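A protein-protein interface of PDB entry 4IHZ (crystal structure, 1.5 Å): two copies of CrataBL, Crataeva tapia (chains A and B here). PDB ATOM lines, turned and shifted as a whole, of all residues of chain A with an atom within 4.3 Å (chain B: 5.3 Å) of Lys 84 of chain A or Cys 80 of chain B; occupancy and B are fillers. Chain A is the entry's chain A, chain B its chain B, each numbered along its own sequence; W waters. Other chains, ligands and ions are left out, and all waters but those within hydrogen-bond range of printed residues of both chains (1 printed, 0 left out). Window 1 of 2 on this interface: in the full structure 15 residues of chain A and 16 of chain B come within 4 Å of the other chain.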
ATOM      1  N   HIS A  72     -10.370 -19.629  -9.553  1.00  0.00           N
ATOM      2  CA  HIS A  72      -9.194 -20.026  -8.790  1.00  0.00           C
ATOM      3  C   HIS A  72      -8.723 -21.387  -9.171  1.00  0.00           C
ATOM      4  O   HIS A  72      -9.510 -22.229  -9.606  1.00  0.00           O
ATOM      5  CB  HIS A  72      -9.426 -19.900  -7.281  1.00  0.00           C
ATOM      6  CG  HIS A  72     -10.282 -20.961  -6.646  1.00  0.00           C
ATOM      7  ND1 HIS A  72     -11.619 -20.767  -6.389  1.00  0.00           N
ATOM      8  CD2 HIS A  72      -9.963 -22.167  -6.135  1.00  0.00           C
ATOM      9  CE1 HIS A  72     -12.097 -21.825  -5.759  1.00  0.00           C
ATOM     10  NE2 HIS A  72     -11.110 -22.684  -5.576  1.00  0.00           N
ATOM     11  N   THR A  73      -7.429 -21.594  -9.004  1.00  0.00           N
ATOM     12  CA  THR A  73      -6.840 -22.914  -9.301  1.00  0.00           C
ATOM     13  C   THR A  73      -7.228 -23.913  -8.217  1.00  0.00           C
ATOM     14  O   THR A  73      -7.197 -23.589  -7.012  1.00  0.00           O
ATOM     15  CB  THR A  73      -5.333 -22.784  -9.453  1.00  0.00           C
ATOM     16  OG1 THR A  73      -5.062 -22.116 -10.682  1.00  0.00           O
ATOM     17  CG2 THR A  73      -4.598 -24.127  -9.459  1.00  0.00           C
ATOM     18  N   SER A  75      -5.970 -26.958  -6.474  1.00  0.00           N
ATOM     19  CA  SER A  75      -4.729 -27.708  -6.248  1.00  0.00           C
ATOM     20  C   SER A  75      -4.476 -27.744  -4.747  1.00  0.00           C
ATOM     21  O   SER A  75      -4.490 -26.689  -4.092  1.00  0.00           O
ATOM     22  CB  SER A  75      -3.530 -27.039  -6.948  1.00  0.00           C
ATOM     23  OG  SER A  75      -2.319 -27.753  -6.698  1.00  0.00           O
ATOM     24  N   TRP A  78       0.640 -25.947  -3.343  1.00  0.00           N
ATOM     25  CA  TRP A  78       0.759 -24.532  -3.763  1.00  0.00           C
ATOM     26  C   TRP A  78       2.080 -24.015  -3.215  1.00  0.00           C
ATOM     27  O   TRP A  78       2.312 -24.042  -2.016  1.00  0.00           O
ATOM     28  CB  TRP A  78      -0.406 -23.716  -3.176  1.00  0.00           C
ATOM     29  CG  TRP A  78      -0.567 -22.442  -3.879  1.00  0.00           C
ATOM     30  CD1 TRP A  78      -0.384 -21.180  -3.385  1.00  0.00           C
ATOM     31  CD2 TRP A  78      -0.945 -22.293  -5.240  1.00  0.00           C
ATOM     32  NE1 TRP A  78      -0.615 -20.251  -4.369  1.00  0.00           N
ATOM     33  CE2 TRP A  78      -0.977 -20.897  -5.524  1.00  0.00           C
ATOM     34  CE3 TRP A  78      -1.291 -23.201  -6.247  1.00  0.00           C
ATOM     35  CZ2 TRP A  78      -1.318 -20.385  -6.793  1.00  0.00           C
ATOM     36  CZ3 TRP A  78      -1.631 -22.682  -7.520  1.00  0.00           C
ATOM     37  CH2 TRP A  78      -1.663 -21.288  -7.764  1.00  0.00           C
ATOM     38  N   GLU A  82       1.173 -16.341  -1.973  1.00  0.00           N
ATOM     39  CA  GLU A  82      -0.037 -15.648  -2.422  1.00  0.00           C
ATOM     40  C   GLU A  82      -1.164 -16.634  -2.818  1.00  0.00           C
ATOM     41  O   GLU A  82      -0.943 -17.862  -2.857  1.00  0.00           O
ATOM     42  CB  GLU A  82       0.297 -14.771  -3.633  1.00  0.00           C
ATOM     43  CG  GLU A  82       1.398 -13.725  -3.366  1.00  0.00           C
ATOM     44  CD  GLU A  82       2.826 -14.225  -3.651  1.00  0.00           C
ATOM     45  OE1 GLU A  82       3.044 -15.440  -3.772  1.00  0.00           O
ATOM     46  OE2 GLU A  82       3.737 -13.376  -3.727  1.00  0.00           O
ATOM     47  N   SER A  83      -2.352 -16.107  -3.090  1.00  0.00           N
ATOM     48  CA  SER A  83      -3.525 -16.956  -3.285  1.00  0.00           C
ATOM     49  C   SER A  83      -3.463 -17.747  -4.617  1.00  0.00           C
ATOM     50  O   SER A  83      -2.649 -17.465  -5.500  1.00  0.00           O
ATOM     51  CB  SER A  83      -4.759 -16.072  -3.357  1.00  0.00           C
ATOM     52  OG  SER A  83      -4.781 -15.453  -4.641  1.00  0.00           O
ATOM     53  N   LYS A  84      -4.455 -18.619  -4.777  1.00  0.00           N
ATOM     54  CA  LYS A  84      -4.690 -19.352  -6.037  1.00  0.00           C
ATOM     55  C   LYS A  84      -5.670 -18.638  -6.959  1.00  0.00           C
ATOM     56  O   LYS A  84      -6.064 -19.193  -7.996  1.00  0.00           O
ATOM     57  CB  LYS A  84      -5.274 -20.717  -5.677  1.00  0.00           C
ATOM     58  CG  LYS A  84      -4.357 -21.565  -4.785  1.00  0.00           C
ATOM     59  CD  LYS A  84      -5.100 -22.762  -4.298  1.00  0.00           C
ATOM     60  CE  LYS A  84      -4.239 -23.591  -3.337  1.00  0.00           C
ATOM     61  NZ  LYS A  84      -5.180 -24.534  -2.753  1.00  0.00           N
ATOM     62  N   ILE A  85      -6.076 -17.432  -6.574  1.00  0.00           N
ATOM     63  CA  ILE A  85      -7.161 -16.744  -7.263  1.00  0.00           C
ATOM     64  C   ILE A  85      -6.584 -15.968  -8.449  1.00  0.00           C
ATOM     65  O   ILE A  85      -5.581 -15.291  -8.341  1.00  0.00           O
ATOM     66  CB  ILE A  85      -7.860 -15.820  -6.269  1.00  0.00           C
ATOM     67  CG1 ILE A  85      -8.476 -16.666  -5.137  1.00  0.00           C
ATOM     68  CG2 ILE A  85      -8.956 -14.924  -6.997  1.00  0.00           C
ATOM     69  CD1 ILE A  85      -8.704 -15.891  -3.854  1.00  0.00           C
ATOM     70  N   TRP A  86      -7.249 -16.085  -9.603  1.00  0.00           N
ATOM     71  CA  TRP A  86      -6.754 -15.401 -10.793  1.00  0.00           C
ATOM     72  C   TRP A  86      -7.024 -13.901 -10.800  1.00  0.00           C
ATOM     73  O   TRP A  86      -8.030 -13.422 -10.274  1.00  0.00           O
ATOM     74  CB  TRP A  86      -7.395 -16.031 -12.011  1.00  0.00           C
ATOM     75  CG  TRP A  86      -6.950 -17.460 -12.255  1.00  0.00           C
ATOM     76  CD1 TRP A  86      -6.433 -18.391 -11.337  1.00  0.00           C
ATOM     77  CD2 TRP A  86      -6.952 -18.122 -13.526  1.00  0.00           C
ATOM     78  NE1 TRP A  86      -6.106 -19.575 -12.009  1.00  0.00           N
ATOM     79  CE2 TRP A  86      -6.451 -19.426 -13.329  1.00  0.00           C
ATOM     80  CE3 TRP A  86      -7.355 -17.727 -14.827  1.00  0.00           C
ATOM     81  CZ2 TRP A  86      -6.295 -20.350 -14.392  1.00  0.00           C
ATOM     82  CZ3 TRP A  86      -7.229 -18.650 -15.863  1.00  0.00           C
ATOM     83  CH2 TRP A  86      -6.710 -19.944 -15.640  1.00  0.00           C
ATOM     84  N   THR A 101      -1.908 -15.702 -10.943  1.00  0.00           N
ATOM     85  CA  THR A 101      -2.610 -16.034  -9.723  1.00  0.00           C
ATOM     86  C   THR A 101      -2.284 -14.945  -8.675  1.00  0.00           C
ATOM     87  O   THR A 101      -1.704 -13.919  -8.995  1.00  0.00           O
ATOM     88  CB  THR A 101      -2.224 -17.432  -9.182  1.00  0.00           C
ATOM     89  OG1 THR A 101      -0.845 -17.413  -8.826  1.00  0.00           O
ATOM     90  CG2 THR A 101      -2.460 -18.562 -10.272  1.00  0.00           C
ATOM     91  N   ASN B  23      -7.028 -24.771   8.033  1.00  0.00           N
ATOM     92  CA  ASN B  23      -7.200 -25.583   6.823  1.00  0.00           C
ATOM     93  C   ASN B  23      -6.222 -26.753   6.728  1.00  0.00           C
ATOM     94  O   ASN B  23      -6.588 -27.825   6.230  1.00  0.00           O
ATOM     95  CB  ASN B  23      -7.151 -24.716   5.557  1.00  0.00           C
ATOM     96  CG  ASN B  23      -5.735 -24.475   5.046  1.00  0.00           C
ATOM     97  OD1 ASN B  23      -5.203 -25.270   4.285  1.00  0.00           O
ATOM     98  ND2 ASN B  23      -5.119 -23.357   5.473  1.00  0.00           N
ATOM     99  N   GLN B  30     -11.252 -26.930   0.376  1.00  0.00           N
ATOM    100  CA  GLN B  30     -12.556 -26.240   0.382  1.00  0.00           C
ATOM    101  C   GLN B  30     -12.643 -25.115  -0.634  1.00  0.00           C
ATOM    102  O   GLN B  30     -11.611 -24.624  -1.080  1.00  0.00           O
ATOM    103  CB  GLN B  30     -12.958 -25.756   1.770  1.00  0.00           C
ATOM    104  CG  GLN B  30     -11.851 -25.130   2.557  1.00  0.00           C
ATOM    105  CD  GLN B  30     -11.081 -26.138   3.376  1.00  0.00           C
ATOM    106  OE1 GLN B  30      -9.853 -26.037   3.505  1.00  0.00           O
ATOM    107  NE2 GLN B  30     -11.799 -27.130   3.948  1.00  0.00           N
ATOM    108  N   CYS B  33     -12.327 -20.164   2.324  1.00  0.00           N
ATOM    109  CA  CYS B  33     -11.934 -20.232   3.724  1.00  0.00           C
ATOM    110  C   CYS B  33     -12.103 -18.839   4.295  1.00  0.00           C
ATOM    111  O   CYS B  33     -11.141 -18.091   4.408  1.00  0.00           O
ATOM    112  CB  CYS B  33     -10.468 -20.668   3.857  1.00  0.00           C
ATOM    113  SG  CYS B  33     -10.170 -22.318   3.246  1.00  0.00           S
ATOM    114  N   ASP B  36      -9.930 -18.590   8.286  1.00  0.00           N
ATOM    115  CA  ASP B  36      -8.960 -19.635   8.510  1.00  0.00           C
ATOM    116  C   ASP B  36      -8.078 -19.264   9.703  1.00  0.00           C
ATOM    117  O   ASP B  36      -7.066 -18.615   9.575  1.00  0.00           O
ATOM    118  CB  ASP B  36      -8.115 -19.814   7.229  1.00  0.00           C
ATOM    119  CG  ASP B  36      -7.248 -21.073   7.271  1.00  0.00           C
ATOM    120  OD1 ASP B  36      -7.735 -22.156   7.709  1.00  0.00           O
ATOM    121  OD2 ASP B  36      -6.070 -20.964   6.880  1.00  0.00           O
ATOM    122  N   TRP B  78      -1.812 -26.624   0.713  1.00  0.00           N
ATOM    123  CA  TRP B  78      -2.696 -25.518   1.078  1.00  0.00           C
ATOM    124  C   TRP B  78      -4.068 -25.832   0.573  1.00  0.00           C
ATOM    125  O   TRP B  78      -4.239 -26.025  -0.609  1.00  0.00           O
ATOM    126  CB  TRP B  78      -2.157 -24.192   0.488  1.00  0.00           C
ATOM    127  CG  TRP B  78      -2.763 -23.022   1.176  1.00  0.00           C
ATOM    128  CD1 TRP B  78      -3.612 -22.087   0.637  1.00  0.00           C
ATOM    129  CD2 TRP B  78      -2.568 -22.641   2.543  1.00  0.00           C
ATOM    130  NE1 TRP B  78      -3.928 -21.130   1.576  1.00  0.00           N
ATOM    131  CE2 TRP B  78      -3.307 -21.441   2.756  1.00  0.00           C
ATOM    132  CE3 TRP B  78      -1.818 -23.172   3.596  1.00  0.00           C
ATOM    133  CZ2 TRP B  78      -3.370 -20.789   4.020  1.00  0.00           C
ATOM    134  CZ3 TRP B  78      -1.825 -22.497   4.835  1.00  0.00           C
ATOM    135  CH2 TRP B  78      -2.614 -21.326   5.030  1.00  0.00           C
ATOM    136  N   PHE B  79      -5.037 -25.914   1.486  1.00  0.00           N
ATOM    137  CA  PHE B  79      -6.387 -26.384   1.142  1.00  0.00           C
ATOM    138  C   PHE B  79      -7.430 -25.268   0.986  1.00  0.00           C
ATOM    139  O   PHE B  79      -8.631 -25.544   0.863  1.00  0.00           O
ATOM    140  CB  PHE B  79      -6.868 -27.411   2.200  1.00  0.00           C
ATOM    141  CG  PHE B  79      -6.001 -28.649   2.281  1.00  0.00           C
ATOM    142  CD1 PHE B  79      -6.082 -29.625   1.290  1.00  0.00           C
ATOM    143  CD2 PHE B  79      -5.136 -28.847   3.342  1.00  0.00           C
ATOM    144  CE1 PHE B  79      -5.290 -30.769   1.356  1.00  0.00           C
ATOM    145  CE2 PHE B  79      -4.345 -29.994   3.422  1.00  0.00           C
ATOM    146  CZ  PHE B  79      -4.422 -30.956   2.416  1.00  0.00           C
ATOM    147  N   CYS B  80      -6.987 -24.021   0.967  1.00  0.00           N
ATOM    148  CA  CYS B  80      -7.864 -22.879   0.719  1.00  0.00           C
ATOM    149  C   CYS B  80      -7.481 -22.229  -0.599  1.00  0.00           C
ATOM    150  O   CYS B  80      -6.336 -22.343  -1.030  1.00  0.00           O
ATOM    151  CB  CYS B  80      -7.601 -21.826   1.812  1.00  0.00           C
ATOM    152  SG  CYS B  80      -8.114 -22.422   3.417  1.00  0.00           S
ATOM    153  N   PRO B  81      -8.406 -21.522  -1.225  1.00  0.00           N
ATOM    154  CA  PRO B  81      -8.004 -20.722  -2.416  1.00  0.00           C
ATOM    155  C   PRO B  81      -7.271 -19.455  -2.034  1.00  0.00           C
ATOM    156  O   PRO B  81      -6.563 -18.912  -2.887  1.00  0.00           O
ATOM    157  CB  PRO B  81      -9.330 -20.315  -3.083  1.00  0.00           C
ATOM    158  CG  PRO B  81     -10.384 -21.096  -2.357  1.00  0.00           C
ATOM    159  CD  PRO B  81      -9.870 -21.669  -1.105  1.00  0.00           C
ATOM    160  N   GLU B  82      -7.507 -18.960  -0.815  1.00  0.00           N
ATOM    161  CA  GLU B  82      -6.914 -17.679  -0.402  1.00  0.00           C
ATOM    162  C   GLU B  82      -5.431 -17.873  -0.034  1.00  0.00           C
ATOM    163  O   GLU B  82      -4.913 -19.006  -0.005  1.00  0.00           O
ATOM    164  CB  GLU B  82      -7.685 -17.085   0.787  1.00  0.00           C
ATOM    165  CG  GLU B  82      -9.185 -16.876   0.495  1.00  0.00           C
ATOM    166  CD  GLU B  82     -10.102 -18.082   0.791  1.00  0.00           C
ATOM    167  OE1 GLU B  82      -9.603 -19.195   0.923  1.00  0.00           O
ATOM    168  OE2 GLU B  82     -11.341 -17.898   0.904  1.00  0.00           O
HETATM  169  O   HOH W   1     -11.496 -24.915  -4.096  1.00  0.00           O
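The side-chain amino group (NZ) of Lys 84 of chain A lies within hydrogen-bond range of the backbone carbonyl oxygen (O) of Trp 78 of chain B (2.8 Å).
O of Cys 80 of chain B lies within hydrogen-bond range of NZ of Lys 84 of chain A (3.0 Å).
The backbone carbonyl oxygen (O) of Pro 81 of chain B is in hydrogen-bond range of the backbone NH (N) of Lys 84 of chain A.
Of the printed residues of chain B, His 72 of chain A touches Pro 81 (3.6 Å).
Of the printed residues of chain B, Ser 83 of chain A touches Pro 81 (3.4 Å) and Glu 82 (3.8 Å).
Printed residues of chain B within 4 Å of Ile 85 of chain A: Pro 81 (3.7 Å).
Thr 101 of chain A touches none of the printed residues of chain B.
Printed residues of chain A within 4 Å of Trp 78 of chain B: Ser 75 and Lys 84.
Of the printed residues of chain A, Glu 82 of chain B touches Ser 83.
The nearest residue of chain B that does not touch Lys 84 of chain A is Phe 79 of chain B (4.4 Å).
The nearest printed residue of chain A that does not touch Cys 80 of chain B is Ser 75 of chain A (5.6 Å).
CB of Pro 81 of chain B touches CD2 of His 72 of chain A, at 3.6 Å.
Trp 78 of chain B touches Ser 75 of chain A (O to O, 3.6 Å).
Ser 83 of chain A touches Pro 81 of chain B (CB to O, 3.4 Å).
Ser 83 of chain A touches Glu 82 of chain B.
Pro 81 of chain B touches Ile 85 of chain A (O to CG1, 3.7 Å).
The backbone carbonyl oxygen of Lys 84 of chain A sits at hydrogen-bond distance from the backbone NH of Thr 73 of chain A.
The backbone carbonyl oxygen (O) of Ser 75 of chain A sits at hydrogen-bond distance from the side-chain amino group (NZ) of Lys 84 of chain A, at 2.6 Å.
OG of Ser 83 of chain A is in hydrogen-bond range of N of Ile 85 of chain A.
The side-chain sulfur of Cys 33 of chain B is disulfide-bonded to the side-chain sulfur of Cys 80 of chain B (2.1 Å).
The backbone NH (N) of Cys 33 of chain B is in hydrogen-bond range of the side-chain carboxylate (OE2) of Glu 82 of chain B (2.9 Å).
The indole nitrogen (NE1) of Trp 78 of chain B sits at hydrogen-bond distance from the backbone carbonyl oxygen (O) of Glu 82 of chain B (2.8 Å).
Positions printed for both chains: 78 and 82.
Of the 8 pairs that touch across the chains among the printed residues, none has its exchanged pair printed and touching as well.
Hydrophobic or aromatic side chains of chain A that line the printed part of chain B: His 72 and Ile 85.
Printed residues of chain B that touch a printed residue of chain A: Trp 78, Cys 80, Pro 81 and Glu 82.
Hydrophobic or aromatic side chains of chain B that line the printed part of chain A: Pro 81.
Among the printed residues, 8 pairs touch across the chains.
Water W1 lies within hydrogen-bond range of NE2 of His 72 of chain A (2.7 Å) and O of Gln 30 of chain B (3.0 Å).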
